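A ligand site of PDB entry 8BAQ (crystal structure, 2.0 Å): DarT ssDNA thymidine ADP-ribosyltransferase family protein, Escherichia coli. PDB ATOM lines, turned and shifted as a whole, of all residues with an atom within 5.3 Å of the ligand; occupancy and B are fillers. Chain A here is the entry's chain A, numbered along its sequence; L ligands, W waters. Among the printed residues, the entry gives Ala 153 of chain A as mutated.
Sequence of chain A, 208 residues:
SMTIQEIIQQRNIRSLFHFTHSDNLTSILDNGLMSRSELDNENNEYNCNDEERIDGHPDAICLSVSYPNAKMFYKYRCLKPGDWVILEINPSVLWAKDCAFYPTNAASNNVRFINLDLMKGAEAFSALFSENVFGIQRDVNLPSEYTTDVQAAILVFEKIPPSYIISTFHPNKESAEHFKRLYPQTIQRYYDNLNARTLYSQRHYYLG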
ATOM      1  N   PHE A  17      32.092  23.570 -16.230  1.00  0.00           N
ATOM      2  CA  PHE A  17      31.270  24.653 -15.687  1.00  0.00           C
ATOM      3  C   PHE A  17      30.897  24.378 -14.239  1.00  0.00           C
ATOM      4  O   PHE A  17      30.719  23.231 -13.815  1.00  0.00           O
ATOM      5  CB  PHE A  17      30.022  24.870 -16.549  1.00  0.00           C
ATOM      6  CG  PHE A  17      30.321  25.525 -17.870  1.00  0.00           C
ATOM      7  CD1 PHE A  17      30.765  26.832 -17.928  1.00  0.00           C
ATOM      8  CD2 PHE A  17      30.189  24.825 -19.066  1.00  0.00           C
ATOM      9  CE1 PHE A  17      31.056  27.433 -19.145  1.00  0.00           C
ATOM     10  CE2 PHE A  17      30.494  25.428 -20.281  1.00  0.00           C
ATOM     11  CZ  PHE A  17      30.913  26.736 -20.322  1.00  0.00           C
ATOM     12  N   HIS A  18      30.792  25.470 -13.491  1.00  0.00           N
ATOM     13  CA  HIS A  18      30.241  25.425 -12.146  1.00  0.00           C
ATOM     14  C   HIS A  18      29.279  26.600 -11.950  1.00  0.00           C
ATOM     15  O   HIS A  18      29.707  27.761 -11.946  1.00  0.00           O
ATOM     16  CB  HIS A  18      31.374  25.400 -11.116  1.00  0.00           C
ATOM     17  CG  HIS A  18      30.913  25.413  -9.688  1.00  0.00           C
ATOM     18  ND1 HIS A  18      30.636  24.255  -8.984  1.00  0.00           N
ATOM     19  CD2 HIS A  18      30.740  26.429  -8.837  1.00  0.00           C
ATOM     20  CE1 HIS A  18      30.274  24.584  -7.747  1.00  0.00           C
ATOM     21  NE2 HIS A  18      30.332  25.905  -7.639  1.00  0.00           N
ATOM     22  N   PHE A  19      27.991  26.311 -11.757  1.00  0.00           N
ATOM     23  CA  PHE A  19      27.045  27.361 -11.421  1.00  0.00           C
ATOM     24  C   PHE A  19      27.110  27.605  -9.924  1.00  0.00           C
ATOM     25  O   PHE A  19      27.319  26.676  -9.137  1.00  0.00           O
ATOM     26  CB  PHE A  19      25.626  27.027 -11.907  1.00  0.00           C
ATOM     27  CG  PHE A  19      24.963  25.862 -11.214  1.00  0.00           C
ATOM     28  CD1 PHE A  19      24.428  26.002  -9.935  1.00  0.00           C
ATOM     29  CD2 PHE A  19      24.869  24.628 -11.837  1.00  0.00           C
ATOM     30  CE1 PHE A  19      23.830  24.930  -9.302  1.00  0.00           C
ATOM     31  CE2 PHE A  19      24.269  23.554 -11.194  1.00  0.00           C
ATOM     32  CZ  PHE A  19      23.743  23.705  -9.933  1.00  0.00           C
ATOM     33  N   THR A  20      26.919  28.868  -9.546  1.00  0.00           N
ATOM     34  CA  THR A  20      26.839  29.262  -8.155  1.00  0.00           C
ATOM     35  C   THR A  20      26.098  30.600  -8.078  1.00  0.00           C
ATOM     36  O   THR A  20      26.104  31.340  -9.057  1.00  0.00           O
ATOM     37  CB  THR A  20      28.244  29.350  -7.548  1.00  0.00           C
ATOM     38  OG1 THR A  20      28.088  29.500  -6.137  1.00  0.00           O
ATOM     39  CG2 THR A  20      29.061  30.469  -8.141  1.00  0.00           C
ATOM     40  N   HIS A  21      25.481  30.892  -6.926  1.00  0.00           N
ATOM     41  CA  HIS A  21      24.816  32.177  -6.711  1.00  0.00           C
ATOM     42  C   HIS A  21      25.882  33.253  -6.567  1.00  0.00           C
ATOM     43  O   HIS A  21      26.916  33.028  -5.933  1.00  0.00           O
ATOM     44  CB  HIS A  21      23.854  32.088  -5.516  1.00  0.00           C
ATOM     45  CG  HIS A  21      22.939  33.257  -5.374  1.00  0.00           C
ATOM     46  ND1 HIS A  21      23.377  34.536  -5.120  1.00  0.00           N
ATOM     47  CD2 HIS A  21      21.604  33.342  -5.440  1.00  0.00           C
ATOM     48  CE1 HIS A  21      22.343  35.363  -5.049  1.00  0.00           C
ATOM     49  NE2 HIS A  21      21.254  34.651  -5.254  1.00  0.00           N
ATOM     50  N   ASN A  24      28.333  34.110  -3.807  1.00  0.00           N
ATOM     51  CA  ASN A  24      29.480  33.267  -3.476  1.00  0.00           C
ATOM     52  C   ASN A  24      30.732  33.711  -4.215  1.00  0.00           C
ATOM     53  O   ASN A  24      31.842  33.274  -3.871  1.00  0.00           O
ATOM     54  CB  ASN A  24      29.212  31.798  -3.787  1.00  0.00           C
ATOM     55  CG  ASN A  24      28.178  31.157  -2.885  1.00  0.00           C
ATOM     56  OD1 ASN A  24      28.083  31.501  -1.716  1.00  0.00           O
ATOM     57  ND2 ASN A  24      27.401  30.224  -3.414  1.00  0.00           N
ATOM     58  N   SER A  27      34.100  35.252  -2.657  1.00  0.00           N
ATOM     59  CA  SER A  27      34.827  34.294  -1.855  1.00  0.00           C
ATOM     60  C   SER A  27      35.545  33.268  -2.743  1.00  0.00           C
ATOM     61  O   SER A  27      36.641  32.807  -2.414  1.00  0.00           O
ATOM     62  CB  SER A  27      33.855  33.663  -0.900  1.00  0.00           C
ATOM     63  OG  SER A  27      34.481  32.656  -0.130  1.00  0.00           O
ATOM     64  N   ILE A  28      34.909  32.905  -3.865  1.00  0.00           N
ATOM     65  CA  ILE A  28      35.434  31.926  -4.799  1.00  0.00           C
ATOM     66  C   ILE A  28      36.591  32.550  -5.593  1.00  0.00           C
ATOM     67  O   ILE A  28      37.578  31.883  -5.876  1.00  0.00           O
ATOM     68  CB  ILE A  28      34.329  31.396  -5.729  1.00  0.00           C
ATOM     69  CG1 ILE A  28      33.313  30.545  -4.961  1.00  0.00           C
ATOM     70  CG2 ILE A  28      34.912  30.625  -6.903  1.00  0.00           C
ATOM     71  CD1 ILE A  28      32.088  30.159  -5.769  1.00  0.00           C
ATOM     72  N   ASN A  31      39.549  32.856  -2.872  1.00  0.00           N
ATOM     73  CA  ASN A  31      40.076  31.663  -2.231  1.00  0.00           C
ATOM     74  C   ASN A  31      39.976  30.437  -3.149  1.00  0.00           C
ATOM     75  O   ASN A  31      40.540  29.390  -2.842  1.00  0.00           O
ATOM     76  CB  ASN A  31      39.323  31.393  -0.923  1.00  0.00           C
ATOM     77  CG  ASN A  31      39.233  32.615  -0.045  1.00  0.00           C
ATOM     78  OD1 ASN A  31      40.252  33.170   0.364  1.00  0.00           O
ATOM     79  ND2 ASN A  31      38.021  33.080   0.219  1.00  0.00           N
ATOM     80  N   GLY A  32      39.237  30.545  -4.261  1.00  0.00           N
ATOM     81  CA  GLY A  32      38.992  29.398  -5.121  1.00  0.00           C
ATOM     82  C   GLY A  32      37.810  28.549  -4.654  1.00  0.00           C
ATOM     83  O   GLY A  32      37.218  28.811  -3.603  1.00  0.00           O
ATOM     84  N   LEU A  33      37.504  27.519  -5.438  1.00  0.00           N
ATOM     85  CA  LEU A  33      36.403  26.609  -5.139  1.00  0.00           C
ATOM     86  C   LEU A  33      36.818  25.607  -4.064  1.00  0.00           C
ATOM     87  O   LEU A  33      37.912  25.040  -4.125  1.00  0.00           O
ATOM     88  CB  LEU A  33      35.993  25.875  -6.423  1.00  0.00           C
ATOM     89  CG  LEU A  33      35.100  26.669  -7.374  1.00  0.00           C
ATOM     90  CD1 LEU A  33      35.035  26.014  -8.747  1.00  0.00           C
ATOM     91  CD2 LEU A  33      33.713  26.810  -6.778  1.00  0.00           C
ATOM     92  N   MET A  34      35.886  25.366  -3.138  1.00  0.00           N
ATOM     93  CA  MET A  34      36.074  24.441  -2.038  1.00  0.00           C
ATOM     94  C   MET A  34      34.815  23.605  -1.847  1.00  0.00           C
ATOM     95  O   MET A  34      33.717  24.045  -2.179  1.00  0.00           O
ATOM     96  CB  MET A  34      36.336  25.190  -0.724  1.00  0.00           C
ATOM     97  CG  MET A  34      37.702  25.837  -0.636  1.00  0.00           C
ATOM     98  SD  MET A  34      37.841  26.772   0.895  1.00  0.00           S
ATOM     99  CE  MET A  34      38.197  28.408   0.252  1.00  0.00           C
ATOM    100  N   ARG A  36      31.938  21.466   0.493  1.00  0.00           N
ATOM    101  CA  ARG A  36      31.138  21.683   1.689  1.00  0.00           C
ATOM    102  C   ARG A  36      31.922  21.425   2.973  1.00  0.00           C
ATOM    103  O   ARG A  36      31.860  22.218   3.915  1.00  0.00           O
ATOM    104  CB  ARG A  36      29.912  20.758   1.641  1.00  0.00           C
ATOM    105  CG  ARG A  36      28.886  21.130   0.588  1.00  0.00           C
ATOM    106  CD  ARG A  36      28.087  22.333   1.068  1.00  0.00           C
ATOM    107  NE  ARG A  36      27.065  21.958   2.035  1.00  0.00           N
ATOM    108  CZ  ARG A  36      25.877  21.466   1.719  1.00  0.00           C
ATOM    109  NH1 ARG A  36      25.494  21.406   0.459  1.00  0.00           N
ATOM    110  NH2 ARG A  36      25.052  21.043   2.670  1.00  0.00           N
ATOM    111  N   LEU A  39      34.566  24.152   3.441  1.00  0.00           N
ATOM    112  CA  LEU A  39      33.938  25.404   3.810  1.00  0.00           C
ATOM    113  C   LEU A  39      33.525  25.365   5.280  1.00  0.00           C
ATOM    114  O   LEU A  39      33.575  26.390   5.942  1.00  0.00           O
ATOM    115  CB  LEU A  39      32.729  25.656   2.898  1.00  0.00           C
ATOM    116  CG  LEU A  39      33.075  25.962   1.440  1.00  0.00           C
ATOM    117  CD1 LEU A  39      31.818  26.038   0.590  1.00  0.00           C
ATOM    118  CD2 LEU A  39      33.863  27.258   1.322  1.00  0.00           C
ATOM    119  N   GLU A  45      31.301  31.285   5.436  1.00  0.00           N
ATOM    120  CA  GLU A  45      29.935  31.498   4.984  1.00  0.00           C
ATOM    121  C   GLU A  45      29.831  31.142   3.508  1.00  0.00           C
ATOM    122  O   GLU A  45      30.744  31.446   2.739  1.00  0.00           O
ATOM    123  CB  GLU A  45      29.540  32.958   5.160  1.00  0.00           C
ATOM    124  CG  GLU A  45      28.095  33.226   4.794  1.00  0.00           C
ATOM    125  CD  GLU A  45      27.772  34.702   4.637  1.00  0.00           C
ATOM    126  OE1 GLU A  45      26.790  35.158   5.263  1.00  0.00           O
ATOM    127  OE2 GLU A  45      28.522  35.387   3.910  1.00  0.00           O
ATOM    128  N   TYR A  46      28.717  30.519   3.136  1.00  0.00           N
ATOM    129  CA  TYR A  46      28.414  30.233   1.749  1.00  0.00           C
ATOM    130  C   TYR A  46      26.913  30.029   1.562  1.00  0.00           C
ATOM    131  O   TYR A  46      26.203  29.691   2.511  1.00  0.00           O
ATOM    132  CB  TYR A  46      29.165  28.991   1.257  1.00  0.00           C
ATOM    133  CG  TYR A  46      28.968  27.753   2.096  1.00  0.00           C
ATOM    134  CD1 TYR A  46      29.614  27.607   3.321  1.00  0.00           C
ATOM    135  CD2 TYR A  46      28.156  26.723   1.671  1.00  0.00           C
ATOM    136  CE1 TYR A  46      29.453  26.471   4.086  1.00  0.00           C
ATOM    137  CE2 TYR A  46      27.968  25.581   2.431  1.00  0.00           C
ATOM    138  CZ  TYR A  46      28.625  25.453   3.650  1.00  0.00           C
ATOM    139  OH  TYR A  46      28.452  24.315   4.402  1.00  0.00           O
ATOM    140  N   ASN A  47      26.453  30.276   0.327  1.00  0.00           N
ATOM    141  CA  ASN A  47      25.081  30.006  -0.093  1.00  0.00           C
ATOM    142  C   ASN A  47      25.124  28.701  -0.896  1.00  0.00           C
ATOM    143  O   ASN A  47      25.709  28.644  -1.984  1.00  0.00           O
ATOM    144  CB  ASN A  47      24.497  31.230  -0.820  1.00  0.00           C
ATOM    145  CG  ASN A  47      23.190  31.001  -1.562  1.00  0.00           C
ATOM    146  OD1 ASN A  47      22.476  31.968  -1.841  1.00  0.00           O
ATOM    147  ND2 ASN A  47      22.870  29.763  -1.904  1.00  0.00           N
ATOM    148  N   CYS A  48      24.550  27.645  -0.298  1.00  0.00           N
ATOM    149  CA  CYS A  48      24.485  26.327  -0.896  1.00  0.00           C
ATOM    150  C   CYS A  48      23.065  26.013  -1.360  1.00  0.00           C
ATOM    151  O   CYS A  48      22.103  26.677  -0.971  1.00  0.00           O
ATOM    152  CB  CYS A  48      24.968  25.255   0.089  1.00  0.00           C
ATOM    153  SG  CYS A  48      23.885  25.044   1.525  1.00  0.00           S
ATOM    154  N   ASN A  49      22.944  24.954  -2.159  1.00  0.00           N
ATOM    155  CA  ASN A  49      21.734  24.653  -2.904  1.00  0.00           C
ATOM    156  C   ASN A  49      21.154  23.311  -2.464  1.00  0.00           C
ATOM    157  O   ASN A  49      19.943  23.194  -2.290  1.00  0.00           O
ATOM    158  CB  ASN A  49      22.039  24.705  -4.400  1.00  0.00           C
ATOM    159  CG  ASN A  49      22.514  26.073  -4.823  1.00  0.00           C
ATOM    160  OD1 ASN A  49      21.881  27.072  -4.494  1.00  0.00           O
ATOM    161  ND2 ASN A  49      23.646  26.136  -5.505  1.00  0.00           N
ATOM    162  N   ASP A  50      22.035  22.312  -2.295  1.00  0.00           N
ATOM    163  CA  ASP A  50      21.635  20.964  -1.909  1.00  0.00           C
ATOM    164  C   ASP A  50      22.075  20.710  -0.475  1.00  0.00           C
ATOM    165  O   ASP A  50      23.270  20.581  -0.192  1.00  0.00           O
ATOM    166  CB  ASP A  50      22.215  19.968  -2.918  1.00  0.00           C
ATOM    167  CG  ASP A  50      21.983  18.504  -2.591  1.00  0.00           C
ATOM    168  OD1 ASP A  50      21.319  18.207  -1.579  1.00  0.00           O
ATOM    169  OD2 ASP A  50      22.492  17.667  -3.357  1.00  0.00           O
ATOM    170  N   ARG A  53      23.048  16.480   0.347  1.00  0.00           N
ATOM    171  CA  ARG A  53      24.092  15.889  -0.499  1.00  0.00           C
ATOM    172  C   ARG A  53      24.030  14.366  -0.388  1.00  0.00           C
ATOM    173  O   ARG A  53      24.900  13.735   0.212  1.00  0.00           O
ATOM    174  CB  ARG A  53      25.482  16.439  -0.145  1.00  0.00           C
ATOM    175  CG  ARG A  53      25.693  17.907  -0.484  1.00  0.00           C
ATOM    176  CD  ARG A  53      25.757  18.215  -1.966  1.00  0.00           C
ATOM    177  NE  ARG A  53      26.921  17.661  -2.667  1.00  0.00           N
ATOM    178  CZ  ARG A  53      28.143  18.166  -2.670  1.00  0.00           C
ATOM    179  NH1 ARG A  53      28.417  19.296  -2.032  1.00  0.00           N
ATOM    180  NH2 ARG A  53      29.113  17.558  -3.336  1.00  0.00           N
ATOM    181  N   ASP A  55      24.568  12.445  -2.708  1.00  0.00           N
ATOM    182  CA  ASP A  55      25.737  11.936  -3.413  1.00  0.00           C
ATOM    183  C   ASP A  55      26.729  11.378  -2.398  1.00  0.00           C
ATOM    184  O   ASP A  55      27.507  10.492  -2.730  1.00  0.00           O
ATOM    185  CB  ASP A  55      26.418  12.996  -4.279  1.00  0.00           C
ATOM    186  CG  ASP A  55      26.850  14.237  -3.511  1.00  0.00           C
ATOM    187  OD1 ASP A  55      25.985  15.121  -3.304  1.00  0.00           O
ATOM    188  OD2 ASP A  55      28.030  14.321  -3.113  1.00  0.00           O
ATOM    189  N   CYS A  62      31.419  20.028  -7.244  1.00  0.00           N
ATOM    190  CA  CYS A  62      30.692  19.485  -8.381  1.00  0.00           C
ATOM    191  C   CYS A  62      30.842  20.382  -9.615  1.00  0.00           C
ATOM    192  O   CYS A  62      30.517  21.563  -9.574  1.00  0.00           O
ATOM    193  CB  CYS A  62      29.219  19.300  -8.022  1.00  0.00           C
ATOM    194  SG  CYS A  62      28.991  18.414  -6.452  1.00  0.00           S
ATOM    195  N   LEU A  63      31.349  19.798 -10.708  1.00  0.00           N
ATOM    196  CA  LEU A  63      31.470  20.459 -11.985  1.00  0.00           C
ATOM    197  C   LEU A  63      30.726  19.659 -13.054  1.00  0.00           C
ATOM    198  O   LEU A  63      30.412  18.478 -12.848  1.00  0.00           O
ATOM    199  CB  LEU A  63      32.933  20.563 -12.437  1.00  0.00           C
ATOM    200  CG  LEU A  63      33.974  21.006 -11.416  1.00  0.00           C
ATOM    201  CD1 LEU A  63      35.345  20.981 -12.061  1.00  0.00           C
ATOM    202  CD2 LEU A  63      33.660  22.377 -10.850  1.00  0.00           C
ATOM    203  N   SER A  64      30.591  20.289 -14.222  1.00  0.00           N
ATOM    204  CA  SER A  64      30.019  19.685 -15.414  1.00  0.00           C
ATOM    205  C   SER A  64      30.997  19.876 -16.573  1.00  0.00           C
ATOM    206  O   SER A  64      31.818  20.798 -16.558  1.00  0.00           O
ATOM    207  CB  SER A  64      28.661  20.292 -15.766  1.00  0.00           C
ATOM    208  OG  SER A  64      27.723  20.168 -14.704  1.00  0.00           O
ATOM    209  N   ASN A  69      24.692  21.505 -15.556  1.00  0.00           N
ATOM    210  CA  ASN A  69      23.513  20.715 -15.254  1.00  0.00           C
ATOM    211  C   ASN A  69      22.289  21.640 -15.303  1.00  0.00           C
ATOM    212  O   ASN A  69      21.908  22.223 -14.293  1.00  0.00           O
ATOM    213  CB  ASN A  69      23.647  20.012 -13.912  1.00  0.00           C
ATOM    214  CG  ASN A  69      22.450  19.137 -13.613  1.00  0.00           C
ATOM    215  OD1 ASN A  69      21.336  19.445 -14.066  1.00  0.00           O
ATOM    216  ND2 ASN A  69      22.664  18.041 -12.897  1.00  0.00           N
ATOM    217  N   MET A  72      19.191  20.979 -12.716  1.00  0.00           N
ATOM    218  CA  MET A  72      19.354  21.289 -11.308  1.00  0.00           C
ATOM    219  C   MET A  72      19.612  22.781 -11.128  1.00  0.00           C
ATOM    220  O   MET A  72      19.167  23.374 -10.147  1.00  0.00           O
ATOM    221  CB  MET A  72      20.502  20.480 -10.697  1.00  0.00           C
ATOM    222  CG  MET A  72      20.121  19.038 -10.421  1.00  0.00           C
ATOM    223  SD  MET A  72      21.466  18.047  -9.710  1.00  0.00           S
ATOM    224  CE  MET A  72      20.974  17.991  -7.989  1.00  0.00           C
ATOM    225  N   TYR A  76      17.278  25.443  -9.008  1.00  0.00           N
ATOM    226  CA  TYR A  76      17.809  26.266  -7.929  1.00  0.00           C
ATOM    227  C   TYR A  76      17.540  27.740  -8.179  1.00  0.00           C
ATOM    228  O   TYR A  76      17.341  28.487  -7.233  1.00  0.00           O
ATOM    229  CB  TYR A  76      19.303  26.000  -7.718  1.00  0.00           C
ATOM    230  CG  TYR A  76      19.611  24.620  -7.184  1.00  0.00           C
ATOM    231  CD1 TYR A  76      18.900  24.091  -6.126  1.00  0.00           C
ATOM    232  CD2 TYR A  76      20.638  23.854  -7.729  1.00  0.00           C
ATOM    233  CE1 TYR A  76      19.167  22.828  -5.626  1.00  0.00           C
ATOM    234  CE2 TYR A  76      20.916  22.588  -7.247  1.00  0.00           C
ATOM    235  CZ  TYR A  76      20.179  22.074  -6.191  1.00  0.00           C
ATOM    236  OH  TYR A  76      20.414  20.818  -5.685  1.00  0.00           O
ATOM    237  N   ALA A 152      25.505  14.559 -16.077  1.00  0.00           N
ATOM    238  CA  ALA A 152      26.821  13.982 -15.849  1.00  0.00           C
ATOM    239  C   ALA A 152      27.669  14.950 -15.029  1.00  0.00           C
ATOM    240  O   ALA A 152      27.725  16.145 -15.324  1.00  0.00           O
ATOM    241  CB  ALA A 152      27.473  13.669 -17.172  1.00  0.00           C
ATOM    242  N   ALA A 153      28.299  14.428 -13.964  1.00  0.00           N
ATOM    243  CA  ALA A 153      28.983  15.236 -12.975  1.00  0.00           C
ATOM    244  C   ALA A 153      30.450  14.825 -12.847  1.00  0.00           C
ATOM    245  O   ALA A 153      30.808  13.658 -13.044  1.00  0.00           O
ATOM    246  CB  ALA A 153      28.283  15.107 -11.642  1.00  0.00           C
ATOM    247  N   LEU A 155      33.155  15.027  -9.750  1.00  0.00           N
ATOM    248  CA  LEU A 155      33.351  15.315  -8.339  1.00  0.00           C
ATOM    249  C   LEU A 155      34.854  15.472  -8.106  1.00  0.00           C
ATOM    250  O   LEU A 155      35.615  14.521  -8.306  1.00  0.00           O
ATOM    251  CB  LEU A 155      32.782  14.208  -7.461  1.00  0.00           C
ATOM    252  CG  LEU A 155      31.273  13.917  -7.507  1.00  0.00           C
ATOM    253  CD1 LEU A 155      30.768  13.580  -6.108  1.00  0.00           C
ATOM    254  CD2 LEU A 155      30.442  15.032  -8.124  1.00  0.00           C
HETATM  255  P1  LIG L   1      26.225  22.559  -2.733  1.00  0.00           P
HETATM  256  O1  LIG L   1      24.746  22.588  -2.950  1.00  0.00           O
HETATM  257  O2  LIG L   1      26.791  21.553  -1.798  1.00  0.00           O
HETATM  258  O3  LIG L   1      26.676  24.029  -2.290  1.00  0.00           O
HETATM  259  C1  LIG L   1      28.077  24.359  -2.226  1.00  0.00           C
HETATM  260  C2  LIG L   1      28.205  25.800  -2.643  1.00  0.00           C
HETATM  261  O4  LIG L   1      29.481  26.315  -2.187  1.00  0.00           O
HETATM  262  C3  LIG L   1      28.168  26.038  -4.169  1.00  0.00           C
HETATM  263  O5  LIG L   1      27.187  27.008  -4.520  1.00  0.00           O
HETATM  264  C4  LIG L   1      29.600  26.501  -4.470  1.00  0.00           C
HETATM  265  O6  LIG L   1      29.648  27.344  -5.604  1.00  0.00           O
HETATM  266  C5  LIG L   1      29.924  27.214  -3.172  1.00  0.00           C
HETATM  267  N1  LIG L   1      31.328  27.546  -2.963  1.00  0.00           N
HETATM  268  C6  LIG L   1      32.429  26.918  -3.479  1.00  0.00           C
HETATM  269  N2  LIG L   1      33.570  27.470  -3.132  1.00  0.00           N
HETATM  270  C7  LIG L   1      33.196  28.538  -2.327  1.00  0.00           C
HETATM  271  C8  LIG L   1      33.936  29.524  -1.654  1.00  0.00           C
HETATM  272  N3  LIG L   1      35.265  29.583  -1.684  1.00  0.00           N
HETATM  273  N4  LIG L   1      33.255  30.457  -0.944  1.00  0.00           N
HETATM  274  C9  LIG L   1      31.922  30.391  -0.926  1.00  0.00           C
HETATM  275  N5  LIG L   1      31.109  29.505  -1.516  1.00  0.00           N
HETATM  276  C10 LIG L   1      31.812  28.606  -2.229  1.00  0.00           C
HETATM  277  O7  LIG L   1      26.980  22.394  -4.143  1.00  0.00           O
HETATM  278  P2  LIG L   1      26.542  22.657  -5.678  1.00  0.00           P
HETATM  279  O8  LIG L   1      27.780  22.663  -6.514  1.00  0.00           O
HETATM  280  O9  LIG L   1      25.626  23.841  -5.708  1.00  0.00           O
HETATM  281  O10 LIG L   1      25.718  21.341  -6.027  1.00  0.00           O
HETATM  282  C11 LIG L   1      24.292  21.282  -5.829  1.00  0.00           C
HETATM  283  C12 LIG L   1      23.772  20.042  -6.519  1.00  0.00           C
HETATM  284  O11 LIG L   1      23.963  20.186  -7.940  1.00  0.00           O
HETATM  285  C13 LIG L   1      24.470  18.729  -6.151  1.00  0.00           C
HETATM  286  O12 LIG L   1      23.546  17.655  -6.273  1.00  0.00           O
HETATM  287  C14 LIG L   1      25.576  18.599  -7.197  1.00  0.00           C
HETATM  288  O13 LIG L   1      26.043  17.263  -7.429  1.00  0.00           O
HETATM  289  C15 LIG L   1      24.843  19.162  -8.426  1.00  0.00           C
HETATM  290  N6  LIG L   1      25.756  19.734  -9.437  1.00  0.00           N
HETATM  291  C16 LIG L   1      26.174  21.038  -9.347  1.00  0.00           C
HETATM  292  C17 LIG L   1      27.073  21.541 -10.277  1.00  0.00           C
HETATM  293  C18 LIG L   1      27.485  22.978 -10.232  1.00  0.00           C
HETATM  294  O14 LIG L   1      27.730  23.562 -11.295  1.00  0.00           O
HETATM  295  N7  LIG L   1      27.523  23.585  -9.052  1.00  0.00           N
HETATM  296  C19 LIG L   1      27.537  20.731 -11.312  1.00  0.00           C
HETATM  297  C20 LIG L   1      27.111  19.417 -11.384  1.00  0.00           C
HETATM  298  C21 LIG L   1      26.229  18.923 -10.440  1.00  0.00           C
HETATM  299  O   HOH W   1      24.832  28.835  -4.779  1.00  0.00           O
HETATM  300  O   HOH W   2      26.216  26.157  -6.783  1.00  0.00           O
HETATM  301  O   HOH W   3      24.710  16.379 -11.740  1.00  0.00           O
HETATM  302  O   HOH W   4      26.853  22.591 -13.609  1.00  0.00           O
HETATM  303  O   HOH W   5      24.333  15.288  -5.519  1.00  0.00           O
HETATM  304  O   HOH W   6      29.989  21.989  -5.232  1.00  0.00           O
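SD of Met 72 sits close to O11 of the ligand (3.7 Å).
Residues that only touch the ligand: Phe 17 (3.9 Å), Ile 28 (3.3 Å), Leu 33 (3.5 Å), Leu 39 (3.6 Å), Glu 45 (3.99 Å), Tyr 46 (3.4 Å), Cys 48 (3.2 Å), Leu 63 (3.7 Å), Ser 64 (3.4 Å) and Tyr 76 (3.5 Å).
Hydrophobic or aromatic side chains that line the ligand: His 18, Phe 19, Ile 28, Leu 33, Met 34, Leu 39, Tyr 46, Met 72 and Tyr 76.
24 residues have an atom within 4 Å of the ligand: Phe 17, His 18, Phe 19, Thr 20, Asn 24, Ser 27, Ile 28, Gly 32, Leu 33, Met 34, Arg 36, Leu 39, Glu 45, Tyr 46, Asn 47, Cys 48, Asn 49, Asp 50, Arg 53, Cys 62, Leu 63, Ser 64, Met 72 and Tyr 76.
The nearest printed residue that does not touch the ligand is Asn 69 (4.3 Å).
NE2 of His 18 sits at hydrogen-bond distance from O6 of the ligand, 2.6 Å away.
An oxygen (O2) of the ligand is in salt-bridge range of the guanidinium group of Arg 36 (2.6 Å).
The side-chain hydroxyl (OG) of Ser 27 is in hydrogen-bond range of a nitrogen (N4) of the ligand, 2.6 Å away.
OG1 of Thr 20 sits at hydrogen-bond distance from O6 of the ligand (2.7 Å).
NH1 of Arg 53 is in salt-bridge range of O2 of the ligand, at 2.8 Å.
An oxygen (O14) of the ligand sits at hydrogen-bond distance from the backbone NH (N) of Phe 19 (2.8 Å).
A nitrogen (N7) of the ligand is in hydrogen-bond range of the backbone carbonyl oxygen (O) of Phe 19.
The backbone NH of Asp 50 lies within hydrogen-bond range of an oxygen (O1) of the ligand (2.8 Å).
OD2 of Asp 50 lies within hydrogen-bond range of O12 of the ligand, 3.1 Å away.
The backbone carbonyl oxygen of Gly 32 lies within hydrogen-bond range of a nitrogen (N3) of the ligand (2.8 Å).
An oxygen (O1) of the ligand is in hydrogen-bond range of the backbone NH (N) of Asn 49, 3.1 Å away.
An oxygen (O9) of the ligand lies within hydrogen-bond range of the side-chain amide nitrogen (ND2) of Asn 49, 3.0 Å away.
The backbone NH (N) of Met 34 lies within hydrogen-bond range of a nitrogen (N2) of the ligand (3.1 Å).
O13 of the ligand lies within hydrogen-bond range of SG of Cys 62.
O of Asn 47 is in hydrogen-bond range of O5 of the ligand (3.4 Å).
An oxygen (O5) of the ligand sits at hydrogen-bond distance from the side-chain amide nitrogen of Asn 24.
Water W5 bridges O12 of the ligand (2.6 Å) and OD1 of Asp 55 (2.8 Å).
Water W2 lies within hydrogen-bond range of an oxygen (O5) of the ligand (2.6 Å), the backbone carbonyl oxygen of Phe 19 (2.7 Å) and the side-chain amide nitrogen of Asn 49 (2.9 Å).
Water W6 lies within hydrogen-bond range of O8 of the ligand (2.6 Å) and N of Cys 62 (3.2 Å).
Water W4 lies within hydrogen-bond range of O14 of the ligand (2.7 Å), OG of Ser 64 (2.8 Å) and N of Asn 69 (3.1 Å).
The backbone carbonyl oxygen (O) of Cys 62 sits at hydrogen-bond distance from a ring nitrogen (ND1) of His 18, at 2.8 Å.
The side-chain amide nitrogen (ND2) of Asn 31 is in hydrogen-bond range of the backbone carbonyl oxygen (O) of Ser 27 (3.0 Å).
OG1 of Thr 20 sits at hydrogen-bond distance from ND2 of Asn 24 (2.9 Å).
NH2 of Arg 53 is in hydrogen-bond range of SG of Cys 62 (3.2 Å).
The side-chain carboxylate of Asp 55 lies within salt-bridge range of the guanidinium group of Arg 53.
The side-chain amide oxygen (OD1) of Asn 69 is in hydrogen-bond range of the backbone NH (N) of Met 72 (3.0 Å).
O of Asn 47 lies within hydrogen-bond range of ND2 of Asn 24, at 2.7 Å.
The backbone carbonyl oxygen (O) of Ser 64 lies within hydrogen-bond range of the backbone NH (N) of Phe 17, at 2.8 Å.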
